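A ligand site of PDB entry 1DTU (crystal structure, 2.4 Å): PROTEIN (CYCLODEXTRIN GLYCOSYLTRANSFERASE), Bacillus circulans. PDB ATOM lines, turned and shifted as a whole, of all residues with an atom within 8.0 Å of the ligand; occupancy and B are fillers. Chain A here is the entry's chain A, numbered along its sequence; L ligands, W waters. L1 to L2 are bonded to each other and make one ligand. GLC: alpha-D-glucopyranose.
N of Ile 414 lies within hydrogen-bond range of O3 of GLC L1, 2.9 Å away.
The backbone carbonyl oxygen (O) of Ile 414 sits at hydrogen-bond distance from an oxygen (O2) of GLC L1.
O of Gly 446 lies within hydrogen-bond range of O6 of GLC L2.
O2 of GLC L2 lies within hydrogen-bond range of OE2 of Glu 411.
The backbone NH of Ile 414 is in hydrogen-bond range of the side-chain carboxylate of Glu 411 (3.4 Å).
OE2 of Glu 411 lies within hydrogen-bond range of N of Trp 413 (2.7 Å).
OE1 of Glu 411 is in salt-bridge range of NZ of Lys 304, at 3.3 Å.
NE1 of Trp 413 sits at hydrogen-bond distance from O of Ser 445 (2.9 Å).
O of Val 448 lies within hydrogen-bond range of NE of Arg 412 (3.0 Å).
The backbone NH (N) of Arg 412 is in hydrogen-bond range of the backbone carbonyl oxygen (O) of Ile 420, 2.7 Å away.
The backbone NH (N) of Ile 420 sits at hydrogen-bond distance from the backbone carbonyl oxygen (O) of Trp 413 (3.0 Å).
Arg 412 touches the ligand.
CA of Trp 413 touches O3 of GLC L1, 3.6 Å away.
O of Ser 445 touches C6 of GLC L1, at 3.4 Å.
Hydrophobic or aromatic side chains that line the ligand: Trp 413 and Ile 414.
Six residues have an atom within 4 Å of the ligand: Glu 411, Arg 412, Trp 413, Ile 414, Ser 445 and Gly 446.
Water W1 lies within hydrogen-bond range of O of Glu 411 and O3 of GLC L2.
Water W2 lies within hydrogen-bond range of the side-chain hydroxyl of Tyr 301 (2.7 Å), the backbone carbonyl oxygen of Ile 414 (3.0 Å) and an oxygen (O2) of GLC L1 (3.2 Å).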
ATOM      1  N   TYR A 301      -9.866   3.606  -3.964  1.00  0.00           N
ATOM      2  CA  TYR A 301      -9.537   2.859  -2.773  1.00  0.00           C
ATOM      3  C   TYR A 301      -8.130   2.298  -2.874  1.00  0.00           C
ATOM      4  O   TYR A 301      -7.471   2.025  -1.864  1.00  0.00           O
ATOM      5  CB  TYR A 301     -10.576   1.762  -2.499  1.00  0.00           C
ATOM      6  CG  TYR A 301     -11.926   2.338  -2.148  1.00  0.00           C
ATOM      7  CD1 TYR A 301     -12.248   2.602  -0.818  1.00  0.00           C
ATOM      8  CD2 TYR A 301     -12.864   2.630  -3.139  1.00  0.00           C
ATOM      9  CE1 TYR A 301     -13.490   3.141  -0.475  1.00  0.00           C
ATOM     10  CE2 TYR A 301     -14.113   3.172  -2.808  1.00  0.00           C
ATOM     11  CZ  TYR A 301     -14.423   3.426  -1.470  1.00  0.00           C
ATOM     12  OH  TYR A 301     -15.639   3.955  -1.143  1.00  0.00           O
ATOM     13  N   LYS A 304      -5.697   5.300  -2.388  1.00  0.00           N
ATOM     14  CA  LYS A 304      -5.664   5.564  -0.966  1.00  0.00           C
ATOM     15  C   LYS A 304      -4.778   4.563  -0.243  1.00  0.00           C
ATOM     16  O   LYS A 304      -3.998   4.924   0.633  1.00  0.00           O
ATOM     17  CB  LYS A 304      -7.066   5.558  -0.384  1.00  0.00           C
ATOM     18  CG  LYS A 304      -7.063   5.527   1.143  1.00  0.00           C
ATOM     19  CD  LYS A 304      -8.456   5.590   1.743  1.00  0.00           C
ATOM     20  CE  LYS A 304      -8.586   4.758   3.000  1.00  0.00           C
ATOM     21  NZ  LYS A 304      -8.592   5.562   4.229  1.00  0.00           N
ATOM     22  N   GLN A 410      -4.001  12.816   4.660  1.00  0.00           N
ATOM     23  CA  GLN A 410      -5.147  12.191   5.273  1.00  0.00           C
ATOM     24  C   GLN A 410      -6.381  12.180   4.402  1.00  0.00           C
ATOM     25  O   GLN A 410      -6.773  13.215   3.868  1.00  0.00           O
ATOM     26  CB  GLN A 410      -5.491  12.814   6.646  1.00  0.00           C
ATOM     27  CG  GLN A 410      -6.396  11.882   7.479  1.00  0.00           C
ATOM     28  CD  GLN A 410      -7.124  12.613   8.580  1.00  0.00           C
ATOM     29  OE1 GLN A 410      -8.118  12.104   9.139  1.00  0.00           O
ATOM     30  NE2 GLN A 410      -6.626  13.803   8.909  1.00  0.00           N
ATOM     31  N   GLU A 411      -6.974  11.000   4.271  1.00  0.00           N
ATOM     32  CA  GLU A 411      -8.202  10.841   3.502  1.00  0.00           C
ATOM     33  C   GLU A 411      -9.370  11.442   4.267  1.00  0.00           C
ATOM     34  O   GLU A 411      -9.581  11.109   5.432  1.00  0.00           O
ATOM     35  CB  GLU A 411      -8.450   9.358   3.158  1.00  0.00           C
ATOM     36  CG  GLU A 411      -9.821   9.098   2.498  1.00  0.00           C
ATOM     37  CD  GLU A 411     -10.910   8.793   3.492  1.00  0.00           C
ATOM     38  OE1 GLU A 411     -10.780   8.023   4.424  1.00  0.00           O
ATOM     39  OE2 GLU A 411     -12.025   9.428   3.246  1.00  0.00           O
ATOM     40  N   ARG A 412     -10.123  12.336   3.630  1.00  0.00           N
ATOM     41  CA  ARG A 412     -11.246  12.971   4.289  1.00  0.00           C
ATOM     42  C   ARG A 412     -12.586  12.659   3.659  1.00  0.00           C
ATOM     43  O   ARG A 412     -13.648  13.026   4.162  1.00  0.00           O
ATOM     44  CB  ARG A 412     -11.019  14.466   4.429  1.00  0.00           C
ATOM     45  CG  ARG A 412      -9.640  14.783   4.967  1.00  0.00           C
ATOM     46  CD  ARG A 412      -9.638  15.733   6.159  1.00  0.00           C
ATOM     47  NE  ARG A 412     -10.184  15.137   7.375  1.00  0.00           N
ATOM     48  CZ  ARG A 412      -9.936  15.607   8.592  1.00  0.00           C
ATOM     49  NH1 ARG A 412      -9.149  16.662   8.781  1.00  0.00           N
ATOM     50  NH2 ARG A 412     -10.482  15.026   9.650  1.00  0.00           N
ATOM     51  N   TRP A 413     -12.552  11.976   2.524  1.00  0.00           N
ATOM     52  CA  TRP A 413     -13.759  11.609   1.812  1.00  0.00           C
ATOM     53  C   TRP A 413     -13.367  10.722   0.640  1.00  0.00           C
ATOM     54  O   TRP A 413     -12.460  11.044  -0.118  1.00  0.00           O
ATOM     55  CB  TRP A 413     -14.497  12.872   1.337  1.00  0.00           C
ATOM     56  CG  TRP A 413     -15.984  12.741   1.246  1.00  0.00           C
ATOM     57  CD1 TRP A 413     -16.885  13.224   2.130  1.00  0.00           C
ATOM     58  CD2 TRP A 413     -16.746  12.200   0.158  1.00  0.00           C
ATOM     59  NE1 TRP A 413     -18.165  12.992   1.697  1.00  0.00           N
ATOM     60  CE2 TRP A 413     -18.111  12.359   0.489  1.00  0.00           C
ATOM     61  CE3 TRP A 413     -16.417  11.589  -1.050  1.00  0.00           C
ATOM     62  CZ2 TRP A 413     -19.133  11.905  -0.346  1.00  0.00           C
ATOM     63  CZ3 TRP A 413     -17.423  11.142  -1.876  1.00  0.00           C
ATOM     64  CH2 TRP A 413     -18.760  11.298  -1.528  1.00  0.00           C
ATOM     65  N   ILE A 414     -14.033   9.572   0.505  1.00  0.00           N
ATOM     66  CA  ILE A 414     -13.652   8.704  -0.575  1.00  0.00           C
ATOM     67  C   ILE A 414     -14.771   7.820  -1.090  1.00  0.00           C
ATOM     68  O   ILE A 414     -15.688   7.426  -0.366  1.00  0.00           O
ATOM     69  CB  ILE A 414     -12.446   7.859  -0.179  1.00  0.00           C
ATOM     70  CG1 ILE A 414     -11.966   7.006  -1.356  1.00  0.00           C
ATOM     71  CG2 ILE A 414     -12.845   6.936   0.970  1.00  0.00           C
ATOM     72  CD1 ILE A 414     -10.708   6.221  -1.031  1.00  0.00           C
ATOM     73  N   ASN A 415     -14.657   7.483  -2.369  1.00  0.00           N
ATOM     74  CA  ASN A 415     -15.546   6.571  -3.066  1.00  0.00           C
ATOM     75  C   ASN A 415     -14.820   6.006  -4.267  1.00  0.00           C
ATOM     76  O   ASN A 415     -13.616   6.215  -4.409  1.00  0.00           O
ATOM     77  CB  ASN A 415     -16.982   7.083  -3.327  1.00  0.00           C
ATOM     78  CG  ASN A 415     -17.179   7.945  -4.553  1.00  0.00           C
ATOM     79  OD1 ASN A 415     -16.280   8.109  -5.390  1.00  0.00           O
ATOM     80  ND2 ASN A 415     -18.367   8.526  -4.675  1.00  0.00           N
ATOM     81  N   ASN A 416     -15.518   5.298  -5.149  1.00  0.00           N
ATOM     82  CA  ASN A 416     -14.854   4.719  -6.296  1.00  0.00           C
ATOM     83  C   ASN A 416     -14.083   5.725  -7.125  1.00  0.00           C
ATOM     84  O   ASN A 416     -12.951   5.474  -7.518  1.00  0.00           O
ATOM     85  CB  ASN A 416     -15.832   3.964  -7.213  1.00  0.00           C
ATOM     86  CG  ASN A 416     -16.360   2.686  -6.595  1.00  0.00           C
ATOM     87  OD1 ASN A 416     -17.265   2.046  -7.151  1.00  0.00           O
ATOM     88  ND2 ASN A 416     -15.804   2.329  -5.453  1.00  0.00           N
ATOM     89  N   VAL A 418     -14.113   9.364  -6.404  1.00  0.00           N
ATOM     90  CA  VAL A 418     -13.792  10.600  -5.721  1.00  0.00           C
ATOM     91  C   VAL A 418     -12.790  10.429  -4.591  1.00  0.00           C
ATOM     92  O   VAL A 418     -12.837   9.461  -3.822  1.00  0.00           O
ATOM     93  CB  VAL A 418     -15.054  11.278  -5.215  1.00  0.00           C
ATOM     94  CG1 VAL A 418     -14.706  12.490  -4.349  1.00  0.00           C
ATOM     95  CG2 VAL A 418     -15.942  11.705  -6.372  1.00  0.00           C
ATOM     96  N   LEU A 419     -11.879  11.389  -4.479  1.00  0.00           N
ATOM     97  CA  LEU A 419     -10.927  11.396  -3.397  1.00  0.00           C
ATOM     98  C   LEU A 419     -10.632  12.808  -2.930  1.00  0.00           C
ATOM     99  O   LEU A 419     -10.266  13.681  -3.707  1.00  0.00           O
ATOM    100  CB  LEU A 419      -9.615  10.611  -3.652  1.00  0.00           C
ATOM    101  CG  LEU A 419      -8.672  10.680  -2.454  1.00  0.00           C
ATOM    102  CD1 LEU A 419      -9.214   9.827  -1.305  1.00  0.00           C
ATOM    103  CD2 LEU A 419      -7.282  10.204  -2.844  1.00  0.00           C
ATOM    104  N   ILE A 420     -10.814  12.986  -1.626  1.00  0.00           N
ATOM    105  CA  ILE A 420     -10.537  14.247  -0.971  1.00  0.00           C
ATOM    106  C   ILE A 420      -9.519  14.021   0.130  1.00  0.00           C
ATOM    107  O   ILE A 420      -9.767  13.287   1.088  1.00  0.00           O
ATOM    108  CB  ILE A 420     -11.799  14.930  -0.449  1.00  0.00           C
ATOM    109  CG1 ILE A 420     -12.758  15.183  -1.607  1.00  0.00           C
ATOM    110  CG2 ILE A 420     -11.445  16.242   0.225  1.00  0.00           C
ATOM    111  CD1 ILE A 420     -14.088  15.788  -1.163  1.00  0.00           C
ATOM    112  N   SER A 443     -22.006  14.135  -5.198  1.00  0.00           N
ATOM    113  CA  SER A 443     -22.613  14.885  -4.108  1.00  0.00           C
ATOM    114  C   SER A 443     -21.805  14.705  -2.829  1.00  0.00           C
ATOM    115  O   SER A 443     -21.874  13.664  -2.178  1.00  0.00           O
ATOM    116  CB  SER A 443     -24.067  14.523  -3.910  1.00  0.00           C
ATOM    117  OG  SER A 443     -24.653  15.401  -2.972  1.00  0.00           O
ATOM    118  N   ILE A 444     -21.033  15.734  -2.508  1.00  0.00           N
ATOM    119  CA  ILE A 444     -20.176  15.719  -1.333  1.00  0.00           C
ATOM    120  C   ILE A 444     -20.872  16.230  -0.078  1.00  0.00           C
ATOM    121  O   ILE A 444     -21.235  17.401   0.020  1.00  0.00           O
ATOM    122  CB  ILE A 444     -18.861  16.462  -1.536  1.00  0.00           C
ATOM    123  CG1 ILE A 444     -18.171  15.983  -2.805  1.00  0.00           C
ATOM    124  CG2 ILE A 444     -17.968  16.238  -0.329  1.00  0.00           C
ATOM    125  CD1 ILE A 444     -18.170  14.463  -2.955  1.00  0.00           C
ATOM    126  N   SER A 445     -21.024  15.323   0.889  1.00  0.00           N
ATOM    127  CA  SER A 445     -21.627  15.655   2.161  1.00  0.00           C
ATOM    128  C   SER A 445     -20.946  14.917   3.293  1.00  0.00           C
ATOM    129  O   SER A 445     -20.510  13.775   3.131  1.00  0.00           O
ATOM    130  CB  SER A 445     -23.138  15.490   2.181  1.00  0.00           C
ATOM    131  OG  SER A 445     -23.485  14.171   1.818  1.00  0.00           O
ATOM    132  N   GLY A 446     -20.816  15.583   4.437  1.00  0.00           N
ATOM    133  CA  GLY A 446     -20.180  14.991   5.600  1.00  0.00           C
ATOM    134  C   GLY A 446     -18.678  15.177   5.623  1.00  0.00           C
ATOM    135  O   GLY A 446     -17.956  14.524   6.386  1.00  0.00           O
ATOM    136  N   LEU A 447     -18.182  16.073   4.774  1.00  0.00           N
ATOM    137  CA  LEU A 447     -16.767  16.344   4.691  1.00  0.00           C
ATOM    138  C   LEU A 447     -16.291  17.179   5.878  1.00  0.00           C
ATOM    139  O   LEU A 447     -16.791  18.274   6.121  1.00  0.00           O
ATOM    140  CB  LEU A 447     -16.402  17.059   3.375  1.00  0.00           C
ATOM    141  CG  LEU A 447     -14.998  17.646   3.392  1.00  0.00           C
ATOM    142  CD1 LEU A 447     -13.961  16.530   3.369  1.00  0.00           C
ATOM    143  CD2 LEU A 447     -14.799  18.586   2.212  1.00  0.00           C
ATOM    144  N   VAL A 448     -15.308  16.662   6.602  1.00  0.00           N
ATOM    145  CA  VAL A 448     -14.742  17.386   7.717  1.00  0.00           C
ATOM    146  C   VAL A 448     -13.273  17.685   7.458  1.00  0.00           C
ATOM    147  O   VAL A 448     -12.576  16.865   6.882  1.00  0.00           O
ATOM    148  CB  VAL A 448     -14.953  16.679   9.060  1.00  0.00           C
ATOM    149  CG1 VAL A 448     -14.296  17.476  10.177  1.00  0.00           C
ATOM    150  CG2 VAL A 448     -16.444  16.527   9.331  1.00  0.00           C
ATOM    151  N   THR A 449     -12.831  18.863   7.870  1.00  0.00           N
ATOM    152  CA  THR A 449     -11.466  19.274   7.640  1.00  0.00           C
ATOM    153  C   THR A 449     -10.835  20.000   8.812  1.00  0.00           C
ATOM    154  O   THR A 449     -11.426  20.158   9.878  1.00  0.00           O
ATOM    155  CB  THR A 449     -11.344  20.128   6.360  1.00  0.00           C
ATOM    156  OG1 THR A 449     -11.832  21.422   6.624  1.00  0.00           O
ATOM    157  CG2 THR A 449     -12.167  19.490   5.258  1.00  0.00           C
ATOM    158  N   ALA A 476     -16.246  21.388   9.611  1.00  0.00           N
ATOM    159  CA  ALA A 476     -17.266  20.707   8.839  1.00  0.00           C
ATOM    160  C   ALA A 476     -17.656  21.530   7.631  1.00  0.00           C
ATOM    161  O   ALA A 476     -18.114  22.667   7.772  1.00  0.00           O
ATOM    162  CB  ALA A 476     -18.495  20.418   9.699  1.00  0.00           C
HETATM  163  C1  GLC L   1     -19.642   8.875   2.157  1.00  0.00           C
HETATM  164  C2  GLC L   1     -18.202   8.783   1.753  1.00  0.00           C
HETATM  165  C3  GLC L   1     -17.297   8.753   2.965  1.00  0.00           C
HETATM  166  C4  GLC L   1     -17.602   9.948   3.859  1.00  0.00           C
HETATM  167  C5  GLC L   1     -19.085   9.953   4.234  1.00  0.00           C
HETATM  168  C6  GLC L   1     -19.471  11.192   5.001  1.00  0.00           C
HETATM  169  O1  GLC L   1     -20.052   7.688   2.718  1.00  0.00           O
HETATM  170  O2  GLC L   1     -18.008   7.591   0.983  1.00  0.00           O
HETATM  171  O3  GLC L   1     -15.950   8.782   2.523  1.00  0.00           O
HETATM  172  O4  GLC L   1     -16.821   9.771   5.054  1.00  0.00           O
HETATM  173  O5  GLC L   1     -19.848   9.996   3.024  1.00  0.00           O
HETATM  174  O6  GLC L   1     -20.397  10.814   6.024  1.00  0.00           O
HETATM  175  C1  GLC L   2     -15.789  10.700   5.323  1.00  0.00           C
HETATM  176  C2  GLC L   2     -14.548   9.940   5.744  1.00  0.00           C
HETATM  177  C3  GLC L   2     -14.763   9.275   7.082  1.00  0.00           C
HETATM  178  C4  GLC L   2     -15.241  10.279   8.121  1.00  0.00           C
HETATM  179  C5  GLC L   2     -16.468  11.027   7.601  1.00  0.00           C
HETATM  180  C6  GLC L   2     -16.857  12.147   8.505  1.00  0.00           C
HETATM  181  O2  GLC L   2     -14.207   8.976   4.761  1.00  0.00           O
HETATM  182  O3  GLC L   2     -13.551   8.700   7.583  1.00  0.00           O
HETATM  183  O4  GLC L   2     -15.638   9.631   9.314  1.00  0.00           O
HETATM  184  O5  GLC L   2     -16.194  11.611   6.328  1.00  0.00           O
HETATM  185  O6  GLC L   2     -18.198  12.599   8.255  1.00  0.00           O
HETATM  186  O   HOH W   1     -11.360  10.882   7.445  1.00  0.00           O
HETATM  187  O   HOH W   2     -16.260   4.945   1.300  1.00  0.00           O
HETATM  188  O   HOH W   3     -20.241   6.884  -0.367  1.00  0.00           O
HETATM  189  O   HOH W   4     -14.602  13.784   6.565  1.00  0.00           O
